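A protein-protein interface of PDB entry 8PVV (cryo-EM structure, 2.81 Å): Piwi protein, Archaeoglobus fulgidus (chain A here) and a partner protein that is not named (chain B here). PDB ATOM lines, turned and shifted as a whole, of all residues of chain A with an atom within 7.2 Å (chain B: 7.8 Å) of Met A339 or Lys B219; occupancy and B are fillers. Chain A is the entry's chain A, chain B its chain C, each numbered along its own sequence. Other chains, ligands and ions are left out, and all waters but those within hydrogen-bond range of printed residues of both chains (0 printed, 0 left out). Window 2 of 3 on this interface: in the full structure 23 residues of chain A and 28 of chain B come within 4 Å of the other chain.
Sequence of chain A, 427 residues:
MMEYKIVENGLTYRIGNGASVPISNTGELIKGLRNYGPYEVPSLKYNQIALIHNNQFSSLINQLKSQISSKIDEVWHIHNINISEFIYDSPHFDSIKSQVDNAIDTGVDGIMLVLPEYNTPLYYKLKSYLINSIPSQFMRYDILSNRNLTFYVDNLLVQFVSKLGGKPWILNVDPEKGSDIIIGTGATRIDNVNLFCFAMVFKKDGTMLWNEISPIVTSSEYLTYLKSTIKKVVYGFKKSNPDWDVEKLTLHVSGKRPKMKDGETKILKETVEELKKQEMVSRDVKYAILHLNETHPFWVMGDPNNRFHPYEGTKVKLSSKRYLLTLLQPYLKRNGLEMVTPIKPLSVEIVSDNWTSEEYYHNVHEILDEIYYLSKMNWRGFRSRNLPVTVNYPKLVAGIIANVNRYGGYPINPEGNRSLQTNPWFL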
ATOM      1  N   ARG A 307      -1.310 -28.858   9.431  1.00  0.00           N
ATOM      2  CA  ARG A 307      -0.494 -28.466  10.581  1.00  0.00           C
ATOM      3  C   ARG A 307      -1.346 -27.907  11.716  1.00  0.00           C
ATOM      4  O   ARG A 307      -0.902 -27.033  12.463  1.00  0.00           O
ATOM      5  CB  ARG A 307       0.594 -27.466  10.182  1.00  0.00           C
ATOM      6  CG  ARG A 307       1.613 -28.032   9.212  1.00  0.00           C
ATOM      7  CD  ARG A 307       2.834 -28.548   9.947  1.00  0.00           C
ATOM      8  NE  ARG A 307       3.777 -29.208   9.051  1.00  0.00           N
ATOM      9  CZ  ARG A 307       3.655 -30.463   8.633  1.00  0.00           C
ATOM     10  NH1 ARG A 307       2.624 -31.198   9.028  1.00  0.00           N
ATOM     11  NH2 ARG A 307       4.561 -30.984   7.820  1.00  0.00           N
ATOM     12  N   PRO A 330       0.029 -22.619   6.418  1.00  0.00           N
ATOM     13  CA  PRO A 330       1.267 -23.306   6.038  1.00  0.00           C
ATOM     14  C   PRO A 330       1.366 -23.432   4.527  1.00  0.00           C
ATOM     15  O   PRO A 330       0.392 -23.763   3.848  1.00  0.00           O
ATOM     16  CB  PRO A 330       1.138 -24.673   6.717  1.00  0.00           C
ATOM     17  CG  PRO A 330       0.222 -24.426   7.870  1.00  0.00           C
ATOM     18  CD  PRO A 330      -0.757 -23.396   7.392  1.00  0.00           C
ATOM     19  N   TYR A 331       2.555 -23.158   3.999  1.00  0.00           N
ATOM     20  CA  TYR A 331       2.770 -23.169   2.561  1.00  0.00           C
ATOM     21  C   TYR A 331       3.281 -24.525   2.100  1.00  0.00           C
ATOM     22  O   TYR A 331       4.138 -25.132   2.745  1.00  0.00           O
ATOM     23  CB  TYR A 331       3.758 -22.080   2.141  1.00  0.00           C
ATOM     24  CG  TYR A 331       3.233 -20.669   2.274  1.00  0.00           C
ATOM     25  CD1 TYR A 331       1.880 -20.424   2.470  1.00  0.00           C
ATOM     26  CD2 TYR A 331       4.085 -19.580   2.169  1.00  0.00           C
ATOM     27  CE1 TYR A 331       1.398 -19.132   2.585  1.00  0.00           C
ATOM     28  CE2 TYR A 331       3.615 -18.288   2.281  1.00  0.00           C
ATOM     29  CZ  TYR A 331       2.271 -18.069   2.487  1.00  0.00           C
ATOM     30  OH  TYR A 331       1.802 -16.781   2.595  1.00  0.00           O
ATOM     31  N   LYS A 333       5.418 -27.092  -0.231  1.00  0.00           N
ATOM     32  CA  LYS A 333       6.787 -27.071  -0.724  1.00  0.00           C
ATOM     33  C   LYS A 333       6.955 -28.245  -1.679  1.00  0.00           C
ATOM     34  O   LYS A 333       5.999 -28.964  -1.985  1.00  0.00           O
ATOM     35  CB  LYS A 333       7.785 -27.115   0.440  1.00  0.00           C
ATOM     36  CG  LYS A 333       8.226 -25.752   0.936  1.00  0.00           C
ATOM     37  CD  LYS A 333       8.498 -25.767   2.433  1.00  0.00           C
ATOM     38  CE  LYS A 333       9.315 -26.983   2.844  1.00  0.00           C
ATOM     39  NZ  LYS A 333       9.727 -26.917   4.274  1.00  0.00           N
ATOM     40  N   GLY A 336       6.286 -31.035   0.999  1.00  0.00           N
ATOM     41  CA  GLY A 336       5.060 -30.992   1.774  1.00  0.00           C
ATOM     42  C   GLY A 336       4.958 -29.685   2.541  1.00  0.00           C
ATOM     43  O   GLY A 336       5.690 -28.735   2.274  1.00  0.00           O
ATOM     44  N   LEU A 337       4.032 -29.670   3.495  1.00  0.00           N
ATOM     45  CA  LEU A 337       3.842 -28.501   4.340  1.00  0.00           C
ATOM     46  C   LEU A 337       5.068 -28.269   5.215  1.00  0.00           C
ATOM     47  O   LEU A 337       5.809 -29.197   5.544  1.00  0.00           O
ATOM     48  CB  LEU A 337       2.601 -28.672   5.214  1.00  0.00           C
ATOM     49  CG  LEU A 337       1.266 -28.590   4.478  1.00  0.00           C
ATOM     50  CD1 LEU A 337       0.114 -28.726   5.454  1.00  0.00           C
ATOM     51  CD2 LEU A 337       1.169 -27.284   3.714  1.00  0.00           C
ATOM     52  N   GLU A 338       5.277 -27.012   5.592  1.00  0.00           N
ATOM     53  CA  GLU A 338       6.445 -26.623   6.367  1.00  0.00           C
ATOM     54  C   GLU A 338       6.068 -26.422   7.830  1.00  0.00           C
ATOM     55  O   GLU A 338       5.006 -25.875   8.141  1.00  0.00           O
ATOM     56  CB  GLU A 338       7.076 -25.353   5.790  1.00  0.00           C
ATOM     57  CG  GLU A 338       6.154 -24.150   5.719  1.00  0.00           C
ATOM     58  CD  GLU A 338       6.317 -23.222   6.902  1.00  0.00           C
ATOM     59  OE1 GLU A 338       7.377 -23.276   7.560  1.00  0.00           O
ATOM     60  OE2 GLU A 338       5.388 -22.433   7.173  1.00  0.00           O
ATOM     61  N   MET A 339       6.940 -26.892   8.722  1.00  0.00           N
ATOM     62  CA  MET A 339       6.700 -26.775  10.154  1.00  0.00           C
ATOM     63  C   MET A 339       6.565 -25.311  10.550  1.00  0.00           C
ATOM     64  O   MET A 339       7.376 -24.471  10.153  1.00  0.00           O
ATOM     65  CB  MET A 339       7.843 -27.424  10.934  1.00  0.00           C
ATOM     66  CG  MET A 339       8.213 -28.812  10.454  1.00  0.00           C
ATOM     67  SD  MET A 339       6.819 -29.949  10.480  1.00  0.00           S
ATOM     68  CE  MET A 339       7.669 -31.521  10.587  1.00  0.00           C
ATOM     69  N   VAL A 340       5.543 -25.007  11.343  1.00  0.00           N
ATOM     70  CA  VAL A 340       5.240 -23.631  11.705  1.00  0.00           C
ATOM     71  C   VAL A 340       4.934 -23.542  13.193  1.00  0.00           C
ATOM     72  O   VAL A 340       4.440 -24.490  13.810  1.00  0.00           O
ATOM     73  CB  VAL A 340       4.070 -23.071  10.862  1.00  0.00           C
ATOM     74  CG1 VAL A 340       2.737 -23.623  11.338  1.00  0.00           C
ATOM     75  CG2 VAL A 340       4.068 -21.551  10.886  1.00  0.00           C
ATOM     76  N   THR A 341       5.271 -22.394  13.772  1.00  0.00           N
ATOM     77  CA  THR A 341       4.817 -22.054  15.106  1.00  0.00           C
ATOM     78  C   THR A 341       3.305 -21.820  15.073  1.00  0.00           C
ATOM     79  O   THR A 341       2.751 -21.490  14.022  1.00  0.00           O
ATOM     80  CB  THR A 341       5.542 -20.796  15.594  1.00  0.00           C
ATOM     81  OG1 THR A 341       6.925 -20.872  15.228  1.00  0.00           O
ATOM     82  CG2 THR A 341       5.455 -20.641  17.097  1.00  0.00           C
ATOM     83  N   HIS B 212       5.409 -24.408  21.549  1.00  0.00           N
ATOM     84  CA  HIS B 212       5.517 -23.844  20.210  1.00  0.00           C
ATOM     85  C   HIS B 212       6.650 -24.482  19.421  1.00  0.00           C
ATOM     86  O   HIS B 212       6.564 -24.587  18.193  1.00  0.00           O
ATOM     87  CB  HIS B 212       5.726 -22.332  20.293  1.00  0.00           C
ATOM     88  CG  HIS B 212       4.510 -21.577  20.730  1.00  0.00           C
ATOM     89  ND1 HIS B 212       4.143 -20.370  20.174  1.00  0.00           N
ATOM     90  CD2 HIS B 212       3.578 -21.856  21.671  1.00  0.00           C
ATOM     91  CE1 HIS B 212       3.037 -19.939  20.755  1.00  0.00           C
ATOM     92  NE2 HIS B 212       2.676 -20.822  21.667  1.00  0.00           N
ATOM     93  N   LEU B 213       7.706 -24.917  20.106  1.00  0.00           N
ATOM     94  CA  LEU B 213       8.863 -25.538  19.484  1.00  0.00           C
ATOM     95  C   LEU B 213       9.184 -26.838  20.205  1.00  0.00           C
ATOM     96  O   LEU B 213       8.639 -27.138  21.270  1.00  0.00           O
ATOM     97  CB  LEU B 213      10.083 -24.608  19.518  1.00  0.00           C
ATOM     98  CG  LEU B 213       9.937 -23.203  18.938  1.00  0.00           C
ATOM     99  CD1 LEU B 213      11.267 -22.500  18.988  1.00  0.00           C
ATOM    100  CD2 LEU B 213       9.418 -23.245  17.516  1.00  0.00           C
ATOM    101  N   THR B 214      10.077 -27.621  19.606  1.00  0.00           N
ATOM    102  CA  THR B 214      10.536 -28.851  20.227  1.00  0.00           C
ATOM    103  C   THR B 214      11.439 -28.538  21.417  1.00  0.00           C
ATOM    104  O   THR B 214      11.968 -27.431  21.531  1.00  0.00           O
ATOM    105  CB  THR B 214      11.287 -29.712  19.216  1.00  0.00           C
ATOM    106  OG1 THR B 214      12.148 -28.887  18.426  1.00  0.00           O
ATOM    107  CG2 THR B 214      10.322 -30.457  18.312  1.00  0.00           C
ATOM    108  N   GLU B 216      14.378 -29.391  21.831  1.00  0.00           N
ATOM    109  CA  GLU B 216      15.690 -29.038  21.306  1.00  0.00           C
ATOM    110  C   GLU B 216      15.692 -27.718  20.542  1.00  0.00           C
ATOM    111  O   GLU B 216      16.756 -27.284  20.091  1.00  0.00           O
ATOM    112  CB  GLU B 216      16.235 -30.159  20.413  1.00  0.00           C
ATOM    113  CG  GLU B 216      15.495 -30.353  19.102  1.00  0.00           C
ATOM    114  CD  GLU B 216      14.288 -31.258  19.244  1.00  0.00           C
ATOM    115  OE1 GLU B 216      13.850 -31.500  20.389  1.00  0.00           O
ATOM    116  OE2 GLU B 216      13.775 -31.728  18.208  1.00  0.00           O
ATOM    117  N   GLY B 217      14.540 -27.075  20.388  1.00  0.00           N
ATOM    118  CA  GLY B 217      14.477 -25.735  19.840  1.00  0.00           C
ATOM    119  C   GLY B 217      14.066 -25.611  18.388  1.00  0.00           C
ATOM    120  O   GLY B 217      14.328 -24.565  17.786  1.00  0.00           O
ATOM    121  N   LYS B 218      13.436 -26.626  17.811  1.00  0.00           N
ATOM    122  CA  LYS B 218      13.009 -26.595  16.422  1.00  0.00           C
ATOM    123  C   LYS B 218      11.487 -26.568  16.352  1.00  0.00           C
ATOM    124  O   LYS B 218      10.796 -26.981  17.285  1.00  0.00           O
ATOM    125  CB  LYS B 218      13.537 -27.816  15.659  1.00  0.00           C
ATOM    126  CG  LYS B 218      15.063 -27.969  15.602  1.00  0.00           C
ATOM    127  CD  LYS B 218      15.768 -26.943  14.720  1.00  0.00           C
ATOM    128  CE  LYS B 218      16.248 -25.728  15.507  1.00  0.00           C
ATOM    129  NZ  LYS B 218      17.026 -24.786  14.660  1.00  0.00           N
ATOM    130  N   LYS B 219      10.970 -26.075  15.231  1.00  0.00           N
ATOM    131  CA  LYS B 219       9.543 -26.166  14.972  1.00  0.00           C
ATOM    132  C   LYS B 219       9.167 -27.594  14.593  1.00  0.00           C
ATOM    133  O   LYS B 219      10.009 -28.396  14.180  1.00  0.00           O
ATOM    134  CB  LYS B 219       9.123 -25.201  13.862  1.00  0.00           C
ATOM    135  CG  LYS B 219       9.745 -23.824  13.968  1.00  0.00           C
ATOM    136  CD  LYS B 219       9.269 -22.918  12.852  1.00  0.00           C
ATOM    137  CE  LYS B 219       9.822 -21.517  13.019  1.00  0.00           C
ATOM    138  NZ  LYS B 219       9.375 -20.603  11.936  1.00  0.00           N
ATOM    139  N   TYR B 220       7.883 -27.913  14.739  1.00  0.00           N
ATOM    140  CA  TYR B 220       7.425 -29.272  14.496  1.00  0.00           C
ATOM    141  C   TYR B 220       5.954 -29.250  14.107  1.00  0.00           C
ATOM    142  O   TYR B 220       5.273 -28.228  14.216  1.00  0.00           O
ATOM    143  CB  TYR B 220       7.696 -30.155  15.716  1.00  0.00           C
ATOM    144  CG  TYR B 220       6.928 -29.771  16.953  1.00  0.00           C
ATOM    145  CD1 TYR B 220       7.404 -28.792  17.811  1.00  0.00           C
ATOM    146  CD2 TYR B 220       5.766 -30.434  17.303  1.00  0.00           C
ATOM    147  CE1 TYR B 220       6.716 -28.448  18.950  1.00  0.00           C
ATOM    148  CE2 TYR B 220       5.080 -30.103  18.445  1.00  0.00           C
ATOM    149  CZ  TYR B 220       5.559 -29.110  19.266  1.00  0.00           C
ATOM    150  OH  TYR B 220       4.876 -28.771  20.409  1.00  0.00           O
ATOM    151  N   ALA B 221       5.467 -30.403  13.655  1.00  0.00           N
ATOM    152  CA  ALA B 221       4.197 -30.499  12.946  1.00  0.00           C
ATOM    153  C   ALA B 221       2.975 -30.520  13.855  1.00  0.00           C
ATOM    154  O   ALA B 221       1.852 -30.500  13.344  1.00  0.00           O
ATOM    155  CB  ALA B 221       4.186 -31.753  12.068  1.00  0.00           C
ATOM    156  N   THR B 222       3.150 -30.565  15.175  1.00  0.00           N
ATOM    157  CA  THR B 222       2.021 -30.694  16.089  1.00  0.00           C
ATOM    158  C   THR B 222       2.092 -29.669  17.214  1.00  0.00           C
ATOM    159  O   THR B 222       1.649 -29.939  18.332  1.00  0.00           O
ATOM    160  CB  THR B 222       1.948 -32.108  16.664  1.00  0.00           C
ATOM    161  OG1 THR B 222       3.215 -32.455  17.235  1.00  0.00           O
ATOM    162  CG2 THR B 222       1.593 -33.114  15.580  1.00  0.00           C
ATOM    163  N   ALA B 223       2.640 -28.487  16.934  1.00  0.00           N
ATOM    164  CA  ALA B 223       2.830 -27.496  17.987  1.00  0.00           C
ATOM    165  C   ALA B 223       1.506 -26.899  18.444  1.00  0.00           C
ATOM    166  O   ALA B 223       1.326 -26.613  19.633  1.00  0.00           O
ATOM    167  CB  ALA B 223       3.777 -26.398  17.506  1.00  0.00           C
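The side-chain sulfur (SD) of Met A339 lies within hydrogen-bond range of the backbone NH (N) of Ala B221 (3.5 Å).
The guanidinium group (NH2) of Arg A307 is in hydrogen-bond range of the backbone carbonyl oxygen (O) of Leu A337 (3.2 Å). The guanidinium group of Arg A307 is in hydrogen-bond range of the side-chain sulfur of Met A339 (3.4 Å).
Among the printed residues, pairs that only touch across the chains: Arg A307 with Ala B221, Met A339 with Lys B219, Met A339 with Tyr B220, Val A340 with Tyr B220, Thr A341 with His B212 and Thr A341 with Lys B219.
Met A339 touches three residues of chain B. Of chain A, only Met A339 (3.6 Å) and Thr A341 (3.7 Å) come within 4 Å of Lys B219. Printed residues of chain A within 4 Å of Ala B221: Arg A307 (3.5 Å) and Met A339 (3.5 Å). Printed residues of chain A within 4 Å of Tyr B220: Met A339 and Val A340. Pro A330 touches none of the printed residues of chain B. Glu A338 touches none of the printed residues of chain B. The nearest residue of chain B that does not touch Met A339 is Thr B222 (6.0 Å). The nearest residue of chain A that does not touch Lys B219 is Val A340 (4.2 Å). The nearest printed residue of chain A that does not touch Tyr B220 is Arg A307 (4.9 Å).
Hydrophobic or aromatic side chains of chain A within 4 Å of the printed part of chain B: Met A339. Hydrophobic or aromatic side chains of chain B within 4 Å of the printed part of chain A: His B212 and Ala B221. Among the printed residues, 7 pairs touch across the chains.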
